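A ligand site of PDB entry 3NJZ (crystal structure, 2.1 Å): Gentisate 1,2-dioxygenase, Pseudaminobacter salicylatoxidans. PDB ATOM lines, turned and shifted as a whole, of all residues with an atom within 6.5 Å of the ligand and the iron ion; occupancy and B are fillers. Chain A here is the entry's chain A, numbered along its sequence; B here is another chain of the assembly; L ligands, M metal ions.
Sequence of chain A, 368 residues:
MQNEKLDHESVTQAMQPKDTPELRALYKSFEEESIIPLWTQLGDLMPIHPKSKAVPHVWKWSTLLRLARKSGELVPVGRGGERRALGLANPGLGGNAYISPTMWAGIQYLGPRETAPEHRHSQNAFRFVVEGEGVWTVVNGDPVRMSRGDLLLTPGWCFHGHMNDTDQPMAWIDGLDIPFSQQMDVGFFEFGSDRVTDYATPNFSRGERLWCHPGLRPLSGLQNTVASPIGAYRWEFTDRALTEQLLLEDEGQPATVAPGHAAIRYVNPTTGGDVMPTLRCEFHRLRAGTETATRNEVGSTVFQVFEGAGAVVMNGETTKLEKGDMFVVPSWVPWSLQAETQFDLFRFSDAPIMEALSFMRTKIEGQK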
ATOM      1  N   GLU A  82     -13.198   7.665 -22.974  1.00  0.00           N
ATOM      2  CA  GLU A  82     -12.973   8.491 -24.204  1.00  0.00           C
ATOM      3  C   GLU A  82     -11.618   8.365 -24.937  1.00  0.00           C
ATOM      4  O   GLU A  82     -11.567   8.211 -26.170  1.00  0.00           O
ATOM      5  CB  GLU A  82     -13.259   9.978 -23.946  1.00  0.00           C
ATOM      6  CG  GLU A  82     -14.713  10.286 -23.562  1.00  0.00           C
ATOM      7  CD  GLU A  82     -15.705   9.842 -24.634  1.00  0.00           C
ATOM      8  OE1 GLU A  82     -15.666  10.393 -25.777  1.00  0.00           O
ATOM      9  OE2 GLU A  82     -16.526   8.923 -24.322  1.00  0.00           O
ATOM     10  N   ARG A  83     -10.516   8.460 -24.175  1.00  0.00           N
ATOM     11  CA  ARG A  83      -9.183   8.533 -24.747  1.00  0.00           C
ATOM     12  C   ARG A  83      -8.224   7.707 -23.901  1.00  0.00           C
ATOM     13  O   ARG A  83      -8.307   7.717 -22.696  1.00  0.00           O
ATOM     14  CB  ARG A  83      -8.697  10.007 -24.802  1.00  0.00           C
ATOM     15  CG  ARG A  83      -9.664  10.989 -25.514  1.00  0.00           C
ATOM     16  CD  ARG A  83      -9.736  10.698 -27.011  1.00  0.00           C
ATOM     17  NE  ARG A  83     -10.532  11.665 -27.766  1.00  0.00           N
ATOM     18  CZ  ARG A  83     -11.790  11.473 -28.187  1.00  0.00           C
ATOM     19  NH1 ARG A  83     -12.426  10.326 -27.890  1.00  0.00           N
ATOM     20  NH2 ARG A  83     -12.408  12.403 -28.926  1.00  0.00           N
ATOM     21  N   ALA A  85      -5.284   8.353 -22.918  1.00  0.00           N
ATOM     22  CA  ALA A  85      -4.389   9.469 -22.739  1.00  0.00           C
ATOM     23  C   ALA A  85      -3.850   9.451 -21.317  1.00  0.00           C
ATOM     24  O   ALA A  85      -4.613   9.282 -20.342  1.00  0.00           O
ATOM     25  CB  ALA A  85      -5.123  10.822 -23.039  1.00  0.00           C
ATOM     26  N   TRP A 104      -3.058  20.849 -19.258  1.00  0.00           N
ATOM     27  CA  TRP A 104      -2.849  19.409 -19.376  1.00  0.00           C
ATOM     28  C   TRP A 104      -1.832  19.180 -20.493  1.00  0.00           C
ATOM     29  O   TRP A 104      -1.900  19.795 -21.584  1.00  0.00           O
ATOM     30  CB  TRP A 104      -4.164  18.726 -19.696  1.00  0.00           C
ATOM     31  CG  TRP A 104      -4.060  17.324 -20.207  1.00  0.00           C
ATOM     32  CD1 TRP A 104      -3.584  16.914 -21.438  1.00  0.00           C
ATOM     33  CD2 TRP A 104      -4.433  16.132 -19.513  1.00  0.00           C
ATOM     34  NE1 TRP A 104      -3.644  15.525 -21.538  1.00  0.00           N
ATOM     35  CE2 TRP A 104      -4.176  15.031 -20.376  1.00  0.00           C
ATOM     36  CE3 TRP A 104      -4.993  15.889 -18.252  1.00  0.00           C
ATOM     37  CZ2 TRP A 104      -4.461  13.715 -20.008  1.00  0.00           C
ATOM     38  CZ3 TRP A 104      -5.269  14.583 -17.890  1.00  0.00           C
ATOM     39  CH2 TRP A 104      -5.010  13.512 -18.767  1.00  0.00           C
ATOM     40  N   GLY A 106      -0.169  15.552 -22.169  1.00  0.00           N
ATOM     41  CA  GLY A 106      -0.365  14.137 -22.040  1.00  0.00           C
ATOM     42  C   GLY A 106       0.104  13.396 -23.276  1.00  0.00           C
ATOM     43  O   GLY A 106       0.131  13.977 -24.378  1.00  0.00           O
ATOM     44  N   GLN A 108      -0.891  10.319 -25.783  1.00  0.00           N
ATOM     45  CA  GLN A 108      -2.024   9.514 -26.187  1.00  0.00           C
ATOM     46  C   GLN A 108      -1.578   8.421 -27.154  1.00  0.00           C
ATOM     47  O   GLN A 108      -0.699   8.627 -27.990  1.00  0.00           O
ATOM     48  CB  GLN A 108      -3.122  10.369 -26.836  1.00  0.00           C
ATOM     49  CG  GLN A 108      -4.358   9.506 -27.133  1.00  0.00           C
ATOM     50  CD  GLN A 108      -5.620  10.271 -27.421  1.00  0.00           C
ATOM     51  OE1 GLN A 108      -5.728  11.496 -27.179  1.00  0.00           O
ATOM     52  NE2 GLN A 108      -6.612   9.562 -27.928  1.00  0.00           N
ATOM     53  N   ALA A 116     -11.310   6.336 -31.576  1.00  0.00           N
ATOM     54  CA  ALA A 116     -11.661   7.061 -30.340  1.00  0.00           C
ATOM     55  C   ALA A 116     -12.892   7.943 -30.636  1.00  0.00           C
ATOM     56  O   ALA A 116     -12.826   8.777 -31.512  1.00  0.00           O
ATOM     57  CB  ALA A 116     -10.475   7.883 -29.821  1.00  0.00           C
ATOM     58  N   HIS A 119     -16.612  13.651 -29.599  1.00  0.00           N
ATOM     59  CA  HIS A 119     -17.177  14.471 -28.550  1.00  0.00           C
ATOM     60  C   HIS A 119     -16.766  15.944 -28.704  1.00  0.00           C
ATOM     61  O   HIS A 119     -15.955  16.257 -29.574  1.00  0.00           O
ATOM     62  CB  HIS A 119     -16.829  13.906 -27.154  1.00  0.00           C
ATOM     63  CG  HIS A 119     -15.365  13.877 -26.839  1.00  0.00           C
ATOM     64  ND1 HIS A 119     -14.512  14.935 -27.101  1.00  0.00           N
ATOM     65  CD2 HIS A 119     -14.615  12.938 -26.212  1.00  0.00           C
ATOM     66  CE1 HIS A 119     -13.296  14.626 -26.670  1.00  0.00           C
ATOM     67  NE2 HIS A 119     -13.342  13.428 -26.119  1.00  0.00           N
ATOM     68  N   ARG A 120     -17.353  16.841 -27.916  1.00  0.00           N
ATOM     69  CA  ARG A 120     -16.869  18.220 -27.854  1.00  0.00           C
ATOM     70  C   ARG A 120     -16.920  18.782 -26.443  1.00  0.00           C
ATOM     71  O   ARG A 120     -17.663  18.288 -25.591  1.00  0.00           O
ATOM     72  CB  ARG A 120     -17.623  19.128 -28.810  1.00  0.00           C
ATOM     73  CG  ARG A 120     -19.094  19.254 -28.501  1.00  0.00           C
ATOM     74  CD  ARG A 120     -19.682  20.206 -29.488  1.00  0.00           C
ATOM     75  NE  ARG A 120     -21.122  20.314 -29.317  1.00  0.00           N
ATOM     76  CZ  ARG A 120     -21.910  21.112 -30.046  1.00  0.00           C
ATOM     77  NH1 ARG A 120     -23.213  21.125 -29.825  1.00  0.00           N
ATOM     78  NH2 ARG A 120     -21.402  21.880 -30.984  1.00  0.00           N
ATOM     79  N   HIS A 121     -16.105  19.807 -26.190  1.00  0.00           N
ATOM     80  CA  HIS A 121     -15.987  20.380 -24.853  1.00  0.00           C
ATOM     81  C   HIS A 121     -15.453  21.790 -24.953  1.00  0.00           C
ATOM     82  O   HIS A 121     -14.800  22.146 -25.930  1.00  0.00           O
ATOM     83  CB  HIS A 121     -15.090  19.489 -23.963  1.00  0.00           C
ATOM     84  CG  HIS A 121     -13.952  18.868 -24.701  1.00  0.00           C
ATOM     85  ND1 HIS A 121     -12.869  19.607 -25.142  1.00  0.00           N
ATOM     86  CD2 HIS A 121     -13.707  17.592 -25.053  1.00  0.00           C
ATOM     87  CE1 HIS A 121     -12.011  18.803 -25.745  1.00  0.00           C
ATOM     88  NE2 HIS A 121     -12.503  17.576 -25.716  1.00  0.00           N
ATOM     89  N   ALA A 125      -7.927  22.514 -27.310  1.00  0.00           N
ATOM     90  CA  ALA A 125      -7.010  21.382 -27.434  1.00  0.00           C
ATOM     91  C   ALA A 125      -6.181  21.483 -28.698  1.00  0.00           C
ATOM     92  O   ALA A 125      -6.604  22.112 -29.675  1.00  0.00           O
ATOM     93  CB  ALA A 125      -7.771  20.028 -27.407  1.00  0.00           C
ATOM     94  N   ARG A 127      -3.093  18.752 -30.845  1.00  0.00           N
ATOM     95  CA  ARG A 127      -2.245  17.555 -30.898  1.00  0.00           C
ATOM     96  C   ARG A 127      -0.873  17.883 -31.508  1.00  0.00           C
ATOM     97  O   ARG A 127      -0.782  18.605 -32.523  1.00  0.00           O
ATOM     98  CB  ARG A 127      -2.903  16.457 -31.746  1.00  0.00           C
ATOM     99  CG  ARG A 127      -4.430  16.415 -31.734  1.00  0.00           C
ATOM    100  CD  ARG A 127      -4.974  16.021 -30.379  1.00  0.00           C
ATOM    101  NE  ARG A 127      -6.425  16.211 -30.256  1.00  0.00           N
ATOM    102  CZ  ARG A 127      -7.064  16.384 -29.093  1.00  0.00           C
ATOM    103  NH1 ARG A 127      -6.397  16.401 -27.930  1.00  0.00           N
ATOM    104  NH2 ARG A 127      -8.385  16.572 -29.089  1.00  0.00           N
ATOM    105  N   THR A 154      -7.792  21.642 -32.228  1.00  0.00           N
ATOM    106  CA  THR A 154      -9.159  21.281 -31.937  1.00  0.00           C
ATOM    107  C   THR A 154      -9.769  22.312 -30.967  1.00  0.00           C
ATOM    108  O   THR A 154      -9.906  22.066 -29.751  1.00  0.00           O
ATOM    109  CB  THR A 154      -9.256  19.858 -31.390  1.00  0.00           C
ATOM    110  OG1 THR A 154      -8.798  18.955 -32.407  1.00  0.00           O
ATOM    111  CG2 THR A 154     -10.693  19.536 -31.059  1.00  0.00           C
ATOM    112  N   HIS A 160     -14.747  16.316 -32.193  1.00  0.00           N
ATOM    113  CA  HIS A 160     -13.552  15.610 -32.667  1.00  0.00           C
ATOM    114  C   HIS A 160     -13.553  14.134 -32.240  1.00  0.00           C
ATOM    115  O   HIS A 160     -14.022  13.794 -31.137  1.00  0.00           O
ATOM    116  CB  HIS A 160     -12.249  16.295 -32.211  1.00  0.00           C
ATOM    117  CG  HIS A 160     -12.152  16.473 -30.722  1.00  0.00           C
ATOM    118  ND1 HIS A 160     -12.914  17.406 -30.045  1.00  0.00           N
ATOM    119  CD2 HIS A 160     -11.403  15.835 -29.785  1.00  0.00           C
ATOM    120  CE1 HIS A 160     -12.629  17.330 -28.752  1.00  0.00           C
ATOM    121  NE2 HIS A 160     -11.715  16.398 -28.573  1.00  0.00           N
ATOM    122  N   HIS A 162     -10.946  10.359 -33.278  1.00  0.00           N
ATOM    123  CA  HIS A 162      -9.668   9.949 -33.903  1.00  0.00           C
ATOM    124  C   HIS A 162      -9.764   8.478 -34.347  1.00  0.00           C
ATOM    125  O   HIS A 162     -10.434   7.679 -33.683  1.00  0.00           O
ATOM    126  CB  HIS A 162      -8.450  10.078 -32.951  1.00  0.00           C
ATOM    127  CG  HIS A 162      -8.506  11.208 -31.965  1.00  0.00           C
ATOM    128  ND1 HIS A 162      -8.595  12.542 -32.333  1.00  0.00           N
ATOM    129  CD2 HIS A 162      -8.390  11.211 -30.615  1.00  0.00           C
ATOM    130  CE1 HIS A 162      -8.578  13.306 -31.258  1.00  0.00           C
ATOM    131  NE2 HIS A 162      -8.435  12.526 -30.197  1.00  0.00           N
ATOM    132  N   TRP A 172       0.997  10.411 -29.842  1.00  0.00           N
ATOM    133  CA  TRP A 172       1.198  11.855 -29.999  1.00  0.00           C
ATOM    134  C   TRP A 172       1.047  12.520 -28.622  1.00  0.00           C
ATOM    135  O   TRP A 172       0.753  11.834 -27.609  1.00  0.00           O
ATOM    136  CB  TRP A 172       0.195  12.426 -31.006  1.00  0.00           C
ATOM    137  CG  TRP A 172      -1.267  12.338 -30.605  1.00  0.00           C
ATOM    138  CD1 TRP A 172      -1.989  13.278 -29.925  1.00  0.00           C
ATOM    139  CD2 TRP A 172      -2.180  11.266 -30.876  1.00  0.00           C
ATOM    140  NE1 TRP A 172      -3.290  12.853 -29.749  1.00  0.00           N
ATOM    141  CE2 TRP A 172      -3.426  11.619 -30.330  1.00  0.00           C
ATOM    142  CE3 TRP A 172      -2.051  10.019 -31.520  1.00  0.00           C
ATOM    143  CZ2 TRP A 172      -4.541  10.801 -30.429  1.00  0.00           C
ATOM    144  CZ3 TRP A 172      -3.164   9.182 -31.597  1.00  0.00           C
ATOM    145  CH2 TRP A 172      -4.394   9.585 -31.063  1.00  0.00           C
ATOM    146  N   ASP A 174      -1.049  15.550 -26.451  1.00  0.00           N
ATOM    147  CA  ASP A 174      -2.198  16.413 -26.376  1.00  0.00           C
ATOM    148  C   ASP A 174      -1.863  17.542 -25.443  1.00  0.00           C
ATOM    149  O   ASP A 174      -1.258  17.288 -24.388  1.00  0.00           O
ATOM    150  CB  ASP A 174      -3.343  15.690 -25.718  1.00  0.00           C
ATOM    151  CG  ASP A 174      -3.728  14.457 -26.457  1.00  0.00           C
ATOM    152  OD1 ASP A 174      -4.101  14.578 -27.649  1.00  0.00           O
ATOM    153  OD2 ASP A 174      -3.683  13.371 -25.834  1.00  0.00           O
ATOM    154  N   GLY A 175      -2.270  18.754 -25.803  1.00  0.00           N
ATOM    155  CA  GLY A 175      -2.270  19.885 -24.862  1.00  0.00           C
ATOM    156  C   GLY A 175      -3.683  20.416 -24.740  1.00  0.00           C
ATOM    157  O   GLY A 175      -4.394  20.574 -25.748  1.00  0.00           O
ATOM    158  N   LEU A 176      -4.119  20.698 -23.505  1.00  0.00           N
ATOM    159  CA  LEU A 176      -5.433  21.331 -23.279  1.00  0.00           C
ATOM    160  C   LEU A 176      -5.343  22.336 -22.137  1.00  0.00           C
ATOM    161  O   LEU A 176      -4.421  22.292 -21.317  1.00  0.00           O
ATOM    162  CB  LEU A 176      -6.553  20.322 -22.961  1.00  0.00           C
ATOM    163  CG  LEU A 176      -6.996  19.271 -23.988  1.00  0.00           C
ATOM    164  CD1 LEU A 176      -6.075  18.009 -23.919  1.00  0.00           C
ATOM    165  CD2 LEU A 176      -8.507  18.891 -23.844  1.00  0.00           C
ATOM    166  N   ILE A 178      -7.415  22.136 -19.737  1.00  0.00           N
ATOM    167  CA  ILE A 178      -8.167  21.408 -18.687  1.00  0.00           C
ATOM    168  C   ILE A 178      -7.987  21.956 -17.246  1.00  0.00           C
ATOM    169  O   ILE A 178      -8.987  22.196 -16.570  1.00  0.00           O
ATOM    170  CB  ILE A 178      -7.866  19.873 -18.751  1.00  0.00           C
ATOM    171  CG1 ILE A 178      -8.721  19.213 -19.837  1.00  0.00           C
ATOM    172  CG2 ILE A 178      -8.103  19.163 -17.394  1.00  0.00           C
ATOM    173  CD1 ILE A 178      -8.193  17.818 -20.239  1.00  0.00           C
ATOM    174  N   PHE A 189     -19.346  19.803 -21.748  1.00  0.00           N
ATOM    175  CA  PHE A 189     -18.955  18.593 -22.479  1.00  0.00           C
ATOM    176  C   PHE A 189     -20.175  17.987 -23.127  1.00  0.00           C
ATOM    177  O   PHE A 189     -21.265  17.972 -22.514  1.00  0.00           O
ATOM    178  CB  PHE A 189     -18.354  17.573 -21.525  1.00  0.00           C
ATOM    179  CG  PHE A 189     -17.793  16.350 -22.206  1.00  0.00           C
ATOM    180  CD1 PHE A 189     -18.628  15.283 -22.573  1.00  0.00           C
ATOM    181  CD2 PHE A 189     -16.412  16.243 -22.450  1.00  0.00           C
ATOM    182  CE1 PHE A 189     -18.106  14.120 -23.199  1.00  0.00           C
ATOM    183  CE2 PHE A 189     -15.881  15.084 -23.074  1.00  0.00           C
ATOM    184  CZ  PHE A 189     -16.731  14.032 -23.453  1.00  0.00           C
ATOM    185  N   LEU B  38      -6.283   9.534 -18.202  1.00  0.00           N
ATOM    186  CA  LEU B  38      -7.533  10.291 -18.392  1.00  0.00           C
ATOM    187  C   LEU B  38      -8.753   9.437 -18.102  1.00  0.00           C
ATOM    188  O   LEU B  38      -9.761   9.928 -17.541  1.00  0.00           O
ATOM    189  CB  LEU B  38      -7.632  10.834 -19.819  1.00  0.00           C
ATOM    190  CG  LEU B  38      -8.878  11.666 -20.103  1.00  0.00           C
ATOM    191  CD1 LEU B  38      -8.838  12.991 -19.329  1.00  0.00           C
ATOM    192  CD2 LEU B  38      -8.986  11.930 -21.609  1.00  0.00           C
ATOM    193  N   LEU B  42     -12.142  11.151 -16.413  1.00  0.00           N
ATOM    194  CA  LEU B  42     -12.730  12.023 -17.442  1.00  0.00           C
ATOM    195  C   LEU B  42     -13.874  12.931 -16.972  1.00  0.00           C
ATOM    196  O   LEU B  42     -13.853  14.134 -17.252  1.00  0.00           O
ATOM    197  CB  LEU B  42     -13.128  11.228 -18.717  1.00  0.00           C
ATOM    198  CG  LEU B  42     -13.460  12.149 -19.915  1.00  0.00           C
ATOM    199  CD1 LEU B  42     -12.580  11.927 -21.118  1.00  0.00           C
ATOM    200  CD2 LEU B  42     -14.910  12.113 -20.314  1.00  0.00           C
ATOM    201  N   MET B  46     -13.803  16.958 -16.939  1.00  0.00           N
ATOM    202  CA  MET B  46     -14.545  17.579 -18.049  1.00  0.00           C
ATOM    203  C   MET B  46     -16.064  17.416 -17.917  1.00  0.00           C
ATOM    204  O   MET B  46     -16.673  16.626 -18.624  1.00  0.00           O
ATOM    205  CB  MET B  46     -14.032  17.017 -19.400  1.00  0.00           C
ATOM    206  CG  MET B  46     -12.488  17.074 -19.546  1.00  0.00           C
ATOM    207  SD  MET B  46     -11.869  16.614 -21.178  1.00  0.00           S
ATOM    208  CE  MET B  46     -11.975  18.181 -21.991  1.00  0.00           C
HETATM  209  C1  LIG L   1      -8.770  14.121 -26.858  1.00  0.00           C
HETATM  210  O1  LIG L   1      -8.024  13.397 -27.592  1.00  0.00           O
HETATM  211  O2  LIG L   1      -9.873  14.568 -27.262  1.00  0.00           O
HETATM  212  C2  LIG L   1      -8.307  14.437 -25.459  1.00  0.00           C
HETATM  213  C3  LIG L   1      -9.230  15.109 -24.514  1.00  0.00           C
HETATM  214  C4  LIG L   1      -8.750  15.373 -23.227  1.00  0.00           C
HETATM  215  C5  LIG L   1      -7.428  15.006 -22.855  1.00  0.00           C
HETATM  216  C6  LIG L   1      -6.567  14.376 -23.759  1.00  0.00           C
HETATM  217  C7  LIG L   1      -7.019  14.100 -25.046  1.00  0.00           C
HETATM  218  O3  LIG L   1     -10.511  15.454 -24.881  1.00  0.00           O
HETATM  219 FE    FE M   1     -11.450  15.833 -26.535  1.00  0.00          FE
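The iron ion is bound by O3 of the ligand (1.9 Å), NE2 of His 160 (2.1 Å), O2 of the ligand (2.1 Å) and NE2 of His 121 (2.2 Å).
An oxygen (O1) of the ligand is in salt-bridge range of the guanidinium group (NE) of Arg 83. NH1 of Arg 127 lies within salt-bridge range of O1 of the ligand (3.4 Å). An oxygen (O1) of the ligand lies close to the side-chain amide oxygen (OE1) of Gln 108 (3.0 Å). A ring nitrogen (NE2) of His 162 lies within hydrogen-bond range of an oxygen (O1) of the ligand, 2.8 Å away.
Merely in contact with the ligand: Ala 85 (3.9 Å), Trp 104 (3.8 Å), His 119 (3.4 Å), Asp 174 (3.5 Å), Leu 176 (3.5 Å), Ile 178 (3.9 Å), Leu 38 of chain B (3.7 Å) and Met 46 of chain B (3.9 Å). Hydrophobic or aromatic side chains within 4 Å of the ligand: Ala 85, His 119, His 121, His 160, His 162, Leu 176, Ile 178, Leu 38 of chain B and Met 46 of chain B. Within 4 Å of the ligand: Arg 83, Ala 85, Trp 104, Gln 108, His 119, His 121, Arg 127, His 160, His 162, Asp 174, Leu 176, Ile 178, Leu 38 of chain B and Met 46 of chain B.
The backbone NH of Ala 116 is in hydrogen-bond range of the backbone carbonyl oxygen of His 162 (2.6 Å). The side-chain amide oxygen (OE1) of Gln 108 lies close to the side-chain carboxylate (OD2) of Asp 174, 3.1 Å away. N of His 160 sits at hydrogen-bond distance from O of His 119 (2.9 Å). O of Leu 176 is in hydrogen-bond range of N of Trp 104, at 2.9 Å. N of Asp 174 lies within hydrogen-bond range of O of Gly 106 (2.9 Å). The backbone carbonyl oxygen (O) of His 160 lies within hydrogen-bond range of the guanidinium group (NH2) of Arg 83 (3.1 Å). NH1 of Arg 127 is in salt-bridge range of OD1 of Asp 174, 2.9 Å away. A ring nitrogen (NE2) of His 162 is in hydrogen-bond range of the guanidinium group (NE) of Arg 83, 3.3 Å away.
Residues that only touch the iron ion: His 119 (2.2 Å). Of the 24 residues printed, 3 come within 4 Å of the iron ion.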
